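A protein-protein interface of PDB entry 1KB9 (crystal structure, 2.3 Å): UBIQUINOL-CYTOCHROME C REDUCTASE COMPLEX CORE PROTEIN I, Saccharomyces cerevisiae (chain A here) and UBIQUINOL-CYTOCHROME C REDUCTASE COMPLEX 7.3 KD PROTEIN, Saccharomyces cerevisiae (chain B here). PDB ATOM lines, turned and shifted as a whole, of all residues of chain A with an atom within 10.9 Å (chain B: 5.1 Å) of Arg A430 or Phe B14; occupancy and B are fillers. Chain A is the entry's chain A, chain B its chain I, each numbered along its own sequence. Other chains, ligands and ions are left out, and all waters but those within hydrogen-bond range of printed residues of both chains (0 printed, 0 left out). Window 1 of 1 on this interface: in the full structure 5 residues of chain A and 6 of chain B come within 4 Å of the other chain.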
ATOM      1  N   LYS A 323     -22.002  15.753 -31.021  1.00  0.00           N
ATOM      2  CA  LYS A 323     -22.078  17.088 -30.429  1.00  0.00           C
ATOM      3  C   LYS A 323     -23.082  17.915 -31.248  1.00  0.00           C
ATOM      4  O   LYS A 323     -23.849  18.697 -30.692  1.00  0.00           O
ATOM      5  CB  LYS A 323     -20.711  17.788 -30.410  1.00  0.00           C
ATOM      6  CG  LYS A 323     -19.726  17.281 -29.351  1.00  0.00           C
ATOM      7  CD  LYS A 323     -20.281  17.320 -27.923  1.00  0.00           C
ATOM      8  CE  LYS A 323     -20.770  15.946 -27.466  1.00  0.00           C
ATOM      9  NZ  LYS A 323     -21.207  15.920 -26.025  1.00  0.00           N
ATOM     10  N   ASN A 326     -26.517  17.074 -30.326  1.00  0.00           N
ATOM     11  CA  ASN A 326     -26.858  17.627 -29.011  1.00  0.00           C
ATOM     12  C   ASN A 326     -27.544  18.967 -29.220  1.00  0.00           C
ATOM     13  O   ASN A 326     -28.430  19.355 -28.459  1.00  0.00           O
ATOM     14  CB  ASN A 326     -25.614  17.894 -28.152  1.00  0.00           C
ATOM     15  CG  ASN A 326     -24.941  16.630 -27.640  1.00  0.00           C
ATOM     16  OD1 ASN A 326     -23.766  16.661 -27.306  1.00  0.00           O
ATOM     17  ND2 ASN A 326     -25.677  15.527 -27.566  1.00  0.00           N
ATOM     18  N   THR A 329     -31.469  19.775 -29.247  1.00  0.00           N
ATOM     19  CA  THR A 329     -32.228  19.933 -28.015  1.00  0.00           C
ATOM     20  C   THR A 329     -32.051  21.315 -27.413  1.00  0.00           C
ATOM     21  O   THR A 329     -32.976  21.859 -26.805  1.00  0.00           O
ATOM     22  CB  THR A 329     -31.798  18.895 -26.950  1.00  0.00           C
ATOM     23  OG1 THR A 329     -32.029  17.575 -27.441  1.00  0.00           O
ATOM     24  CG2 THR A 329     -32.574  19.070 -25.648  1.00  0.00           C
ATOM     25  N   ILE A 330     -30.893  21.915 -27.652  1.00  0.00           N
ATOM     26  CA  ILE A 330     -30.599  23.197 -27.033  1.00  0.00           C
ATOM     27  C   ILE A 330     -30.360  24.447 -27.874  1.00  0.00           C
ATOM     28  O   ILE A 330     -30.694  25.545 -27.426  1.00  0.00           O
ATOM     29  CB  ILE A 330     -29.384  23.052 -26.090  1.00  0.00           C
ATOM     30  CG1 ILE A 330     -28.132  22.723 -26.904  1.00  0.00           C
ATOM     31  CG2 ILE A 330     -29.628  21.945 -25.070  1.00  0.00           C
ATOM     32  CD1 ILE A 330     -26.845  22.783 -26.107  1.00  0.00           C
ATOM     33  N   TRP A 401     -31.600  13.258 -26.580  1.00  0.00           N
ATOM     34  CA  TRP A 401     -30.937  13.630 -25.337  1.00  0.00           C
ATOM     35  C   TRP A 401     -30.855  12.582 -24.233  1.00  0.00           C
ATOM     36  O   TRP A 401     -31.857  12.262 -23.584  1.00  0.00           O
ATOM     37  CB  TRP A 401     -31.534  14.926 -24.777  1.00  0.00           C
ATOM     38  CG  TRP A 401     -30.693  15.572 -23.696  1.00  0.00           C
ATOM     39  CD1 TRP A 401     -30.781  15.360 -22.349  1.00  0.00           C
ATOM     40  CD2 TRP A 401     -29.654  16.544 -23.880  1.00  0.00           C
ATOM     41  NE1 TRP A 401     -29.863  16.138 -21.685  1.00  0.00           N
ATOM     42  CE2 TRP A 401     -29.159  16.876 -22.600  1.00  0.00           C
ATOM     43  CE3 TRP A 401     -29.094  17.167 -25.005  1.00  0.00           C
ATOM     44  CZ2 TRP A 401     -28.133  17.803 -22.409  1.00  0.00           C
ATOM     45  CZ3 TRP A 401     -28.068  18.093 -24.816  1.00  0.00           C
ATOM     46  CH2 TRP A 401     -27.600  18.400 -23.525  1.00  0.00           C
ATOM     47  N   ASP A 402     -29.624  12.142 -23.958  1.00  0.00           N
ATOM     48  CA  ASP A 402     -29.342  11.145 -22.926  1.00  0.00           C
ATOM     49  C   ASP A 402     -30.201   9.894 -23.113  1.00  0.00           C
ATOM     50  O   ASP A 402     -30.826   9.398 -22.179  1.00  0.00           O
ATOM     51  CB  ASP A 402     -29.546  11.759 -21.536  1.00  0.00           C
ATOM     52  CG  ASP A 402     -28.999  10.891 -20.419  1.00  0.00           C
ATOM     53  OD1 ASP A 402     -28.085  10.078 -20.655  1.00  0.00           O
ATOM     54  OD2 ASP A 402     -29.484  11.035 -19.283  1.00  0.00           O
ATOM     55  N   SER A 424     -22.167   8.412 -23.649  1.00  0.00           N
ATOM     56  CA  SER A 424     -21.985   9.621 -22.843  1.00  0.00           C
ATOM     57  C   SER A 424     -22.114  10.896 -23.686  1.00  0.00           C
ATOM     58  O   SER A 424     -22.536  11.940 -23.190  1.00  0.00           O
ATOM     59  CB  SER A 424     -20.623   9.593 -22.144  1.00  0.00           C
ATOM     60  OG  SER A 424     -20.582   8.555 -21.177  1.00  0.00           O
ATOM     61  N   MET A 426     -24.260  11.559 -25.819  1.00  0.00           N
ATOM     62  CA  MET A 426     -25.647  11.845 -26.173  1.00  0.00           C
ATOM     63  C   MET A 426     -26.186  13.015 -25.355  1.00  0.00           C
ATOM     64  O   MET A 426     -27.392  13.270 -25.344  1.00  0.00           O
ATOM     65  CB  MET A 426     -26.534  10.611 -25.976  1.00  0.00           C
ATOM     66  CG  MET A 426     -26.240   9.488 -26.929  1.00  0.00           C
ATOM     67  SD  MET A 426     -26.256  10.031 -28.641  1.00  0.00           S
ATOM     68  CE  MET A 426     -27.985   9.970 -28.982  1.00  0.00           C
ATOM     69  N   SER A 427     -25.291  13.697 -24.644  1.00  0.00           N
ATOM     70  CA  SER A 427     -25.658  14.853 -23.829  1.00  0.00           C
ATOM     71  C   SER A 427     -24.448  15.730 -23.522  1.00  0.00           C
ATOM     72  O   SER A 427     -23.343  15.478 -24.008  1.00  0.00           O
ATOM     73  CB  SER A 427     -26.340  14.423 -22.528  1.00  0.00           C
ATOM     74  OG  SER A 427     -25.470  13.678 -21.701  1.00  0.00           O
ATOM     75  N   MET A 428     -24.676  16.783 -22.743  1.00  0.00           N
ATOM     76  CA  MET A 428     -23.620  17.710 -22.365  1.00  0.00           C
ATOM     77  C   MET A 428     -23.725  18.089 -20.901  1.00  0.00           C
ATOM     78  O   MET A 428     -24.818  18.103 -20.327  1.00  0.00           O
ATOM     79  CB  MET A 428     -23.712  18.998 -23.184  1.00  0.00           C
ATOM     80  CG  MET A 428     -23.511  18.849 -24.672  1.00  0.00           C
ATOM     81  SD  MET A 428     -23.686  20.455 -25.462  1.00  0.00           S
ATOM     82  CE  MET A 428     -21.982  21.036 -25.367  1.00  0.00           C
ATOM     83  N   MET A 429     -22.582  18.436 -20.316  1.00  0.00           N
ATOM     84  CA  MET A 429     -22.505  18.871 -18.925  1.00  0.00           C
ATOM     85  C   MET A 429     -23.075  20.292 -18.869  1.00  0.00           C
ATOM     86  O   MET A 429     -22.929  21.065 -19.818  1.00  0.00           O
ATOM     87  CB  MET A 429     -21.042  18.908 -18.464  1.00  0.00           C
ATOM     88  CG  MET A 429     -20.293  17.574 -18.492  1.00  0.00           C
ATOM     89  SD  MET A 429     -20.771  16.447 -17.172  1.00  0.00           S
ATOM     90  CE  MET A 429     -19.977  17.217 -15.759  1.00  0.00           C
ATOM     91  N   ARG A 430     -23.714  20.633 -17.758  1.00  0.00           N
ATOM     92  CA  ARG A 430     -24.290  21.965 -17.571  1.00  0.00           C
ATOM     93  C   ARG A 430     -24.406  22.290 -16.082  1.00  0.00           C
ATOM     94  O   ARG A 430     -24.373  21.390 -15.236  1.00  0.00           O
ATOM     95  CB  ARG A 430     -25.664  22.052 -18.254  1.00  0.00           C
ATOM     96  CG  ARG A 430     -26.625  20.940 -17.863  1.00  0.00           C
ATOM     97  CD  ARG A 430     -27.923  20.977 -18.661  1.00  0.00           C
ATOM     98  NE  ARG A 430     -28.739  22.161 -18.384  1.00  0.00           N
ATOM     99  CZ  ARG A 430     -29.244  22.477 -17.193  1.00  0.00           C
ATOM    100  NH1 ARG A 430     -29.975  23.576 -17.054  1.00  0.00           N
ATOM    101  NH2 ARG A 430     -29.013  21.711 -16.133  1.00  0.00           N
ATOM    102  N   TRP A 431     -24.510  23.576 -15.758  1.00  0.00           N
ATOM    103  CA  TRP A 431     -24.638  23.997 -14.363  1.00  0.00           C
ATOM    104  C   TRP A 431     -26.060  23.755 -13.842  1.00  0.00           C
ATOM    105  O   TRP A 431     -26.193  23.284 -12.688  1.00  0.00           O
ATOM    106  CB  TRP A 431     -24.254  25.475 -14.203  1.00  0.00           C
ATOM    107  CG  TRP A 431     -24.038  25.887 -12.767  1.00  0.00           C
ATOM    108  CD1 TRP A 431     -24.978  26.377 -11.896  1.00  0.00           C
ATOM    109  CD2 TRP A 431     -22.806  25.826 -12.033  1.00  0.00           C
ATOM    110  NE1 TRP A 431     -24.406  26.619 -10.667  1.00  0.00           N
ATOM    111  CE2 TRP A 431     -23.075  26.289 -10.724  1.00  0.00           C
ATOM    112  CE3 TRP A 431     -21.500  25.424 -12.354  1.00  0.00           C
ATOM    113  CZ2 TRP A 431     -22.087  26.361  -9.735  1.00  0.00           C
ATOM    114  CZ3 TRP A 431     -20.517  25.494 -11.369  1.00  0.00           C
ATOM    115  CH2 TRP A 431     -20.818  25.960 -10.076  1.00  0.00           C
ATOM    116  N   ASN B  11     -33.224  12.987 -15.896  1.00  0.00           N
ATOM    117  CA  ASN B  11     -31.932  13.651 -16.058  1.00  0.00           C
ATOM    118  C   ASN B  11     -31.106  13.536 -14.792  1.00  0.00           C
ATOM    119  O   ASN B  11     -31.649  13.388 -13.697  1.00  0.00           O
ATOM    120  CB  ASN B  11     -32.118  15.127 -16.409  1.00  0.00           C
ATOM    121  CG  ASN B  11     -32.043  15.389 -17.900  1.00  0.00           C
ATOM    122  OD1 ASN B  11     -32.039  16.537 -18.334  1.00  0.00           O
ATOM    123  ND2 ASN B  11     -31.975  14.324 -18.692  1.00  0.00           N
ATOM    124  N   ALA B  12     -29.787  13.594 -14.945  1.00  0.00           N
ATOM    125  CA  ALA B  12     -28.887  13.509 -13.800  1.00  0.00           C
ATOM    126  C   ALA B  12     -28.969  14.792 -12.977  1.00  0.00           C
ATOM    127  O   ALA B  12     -29.456  15.817 -13.456  1.00  0.00           O
ATOM    128  CB  ALA B  12     -27.457  13.271 -14.269  1.00  0.00           C
ATOM    129  N   VAL B  13     -28.547  14.715 -11.717  1.00  0.00           N
ATOM    130  CA  VAL B  13     -28.553  15.881 -10.845  1.00  0.00           C
ATOM    131  C   VAL B  13     -27.395  16.780 -11.281  1.00  0.00           C
ATOM    132  O   VAL B  13     -26.278  16.305 -11.498  1.00  0.00           O
ATOM    133  CB  VAL B  13     -28.400  15.480  -9.370  1.00  0.00           C
ATOM    134  CG1 VAL B  13     -28.549  16.704  -8.472  1.00  0.00           C
ATOM    135  CG2 VAL B  13     -29.440  14.425  -9.012  1.00  0.00           C
ATOM    136  N   PHE B  14     -27.683  18.069 -11.444  1.00  0.00           N
ATOM    137  CA  PHE B  14     -26.694  19.046 -11.896  1.00  0.00           C
ATOM    138  C   PHE B  14     -25.845  19.629 -10.768  1.00  0.00           C
ATOM    139  O   PHE B  14     -26.328  19.786  -9.643  1.00  0.00           O
ATOM    140  CB  PHE B  14     -27.405  20.163 -12.669  1.00  0.00           C
ATOM    141  CG  PHE B  14     -28.366  19.655 -13.714  1.00  0.00           C
ATOM    142  CD1 PHE B  14     -29.730  19.919 -13.609  1.00  0.00           C
ATOM    143  CD2 PHE B  14     -27.914  18.885 -14.782  1.00  0.00           C
ATOM    144  CE1 PHE B  14     -30.630  19.418 -14.554  1.00  0.00           C
ATOM    145  CE2 PHE B  14     -28.803  18.380 -15.732  1.00  0.00           C
ATOM    146  CZ  PHE B  14     -30.164  18.647 -15.615  1.00  0.00           C
ATOM    147  N   VAL B  15     -24.593  19.970 -11.092  1.00  0.00           N
ATOM    148  CA  VAL B  15     -23.631  20.532 -10.126  1.00  0.00           C
ATOM    149  C   VAL B  15     -24.184  21.550  -9.141  1.00  0.00           C
ATOM    150  O   VAL B  15     -23.891  21.467  -7.948  1.00  0.00           O
ATOM    151  CB  VAL B  15     -22.398  21.193 -10.804  1.00  0.00           C
ATOM    152  CG1 VAL B  15     -21.234  20.242 -10.812  1.00  0.00           C
ATOM    153  CG2 VAL B  15     -22.727  21.654 -12.210  1.00  0.00           C
ATOM    154  N   GLY B  16     -24.948  22.520  -9.650  1.00  0.00           N
ATOM    155  CA  GLY B  16     -25.528  23.554  -8.808  1.00  0.00           C
ATOM    156  C   GLY B  16     -26.356  22.977  -7.678  1.00  0.00           C
ATOM    157  O   GLY B  16     -26.210  23.378  -6.521  1.00  0.00           O
ATOM    158  N   THR B  17     -27.201  22.007  -8.012  1.00  0.00           N
ATOM    159  CA  THR B  17     -28.057  21.346  -7.030  1.00  0.00           C
ATOM    160  C   THR B  17     -27.216  20.496  -6.070  1.00  0.00           C
ATOM    161  O   THR B  17     -27.546  20.365  -4.886  1.00  0.00           O
ATOM    162  CB  THR B  17     -29.090  20.444  -7.728  1.00  0.00           C
ATOM    163  OG1 THR B  17     -29.808  21.214  -8.700  1.00  0.00           O
ATOM    164  CG2 THR B  17     -30.069  19.859  -6.715  1.00  0.00           C
ATOM    165  N   ILE B  18     -26.147  19.901  -6.600  1.00  0.00           N
ATOM    166  CA  ILE B  18     -25.236  19.076  -5.818  1.00  0.00           C
ATOM    167  C   ILE B  18     -24.525  19.963  -4.796  1.00  0.00           C
ATOM    168  O   ILE B  18     -24.498  19.646  -3.609  1.00  0.00           O
ATOM    169  CB  ILE B  18     -24.188  18.379  -6.735  1.00  0.00           C
ATOM    170  CG1 ILE B  18     -24.868  17.339  -7.627  1.00  0.00           C
ATOM    171  CG2 ILE B  18     -23.089  17.732  -5.908  1.00  0.00           C
ATOM    172  CD1 ILE B  18     -25.470  16.187  -6.862  1.00  0.00           C
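The backbone carbonyl oxygen (O) of Trp A431 lies within hydrogen-bond range of the backbone NH (N) of Gly B16.
Among the printed residues, pairs that only touch across the chains: Trp A401 with Asn B11 (3.98 Å), Arg A430 with Phe B14 (3.2 Å), Arg A430 with Val B15 (3.5 Å), Trp A431 with Phe B14 (3.3 Å) and Trp A431 with Val B15 (3.7 Å).
Ile A330 touches none of the printed residues of chain B.
Printed residues of chain B within 4 Å of Trp A401: Asn B11.
Ser A427 touches none of the printed residues of chain B.
Arg A430 touches two residues of chain B.
Printed residues of chain B within 4 Å of Trp A431: Phe B14 (3.3 Å), Val B15 (3.7 Å) and Gly B16 (3.4 Å).
Printed residues of chain A within 4 Å of Asn B11: Trp A401.
No residue of chain A comes within 4 Å of Val B13.
Phe B14 touches just these residues of chain A: Arg A430 and Trp A431.
Val B15 touches just these residues of chain A: Arg A430 and Trp A431.
Printed residues of chain A within 4 Å of Gly B16: Trp A431.
No residue of chain A comes within 4 Å of Thr B17.
Ile B18 touches none of the printed residues of chain A.
The nearest printed residue of chain B that does not touch Arg A430 is Gly B16 (5.7 Å).
The nearest printed residue of chain B that does not touch Trp A401 is Phe B14 (6.4 Å).
Of the 8 printed residues of chain B, 4 touch a printed residue of chain A.
Hydrophobic or aromatic side chains of chain B within 4 Å of the printed part of chain A: Phe B14 and Val B15.
Along chain B the printed residues that touch a printed residue of chain A span positions 11 to 16.
Of the 13 printed residues of chain A, 3 touch a printed residue of chain B.
Printed residues of chain A that touch a printed residue of chain B: Trp A401, Arg A430 and Trp A431.
Hydrophobic or aromatic side chains of chain A that line the printed part of chain B: Trp A401 and Trp A431.
Among the printed residues, 6 pairs touch across the chains.
Among the printed residues, no Asp or Glu carboxylate lies within 4 Å of a Lys or Arg side-chain nitrogen of the other chain.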
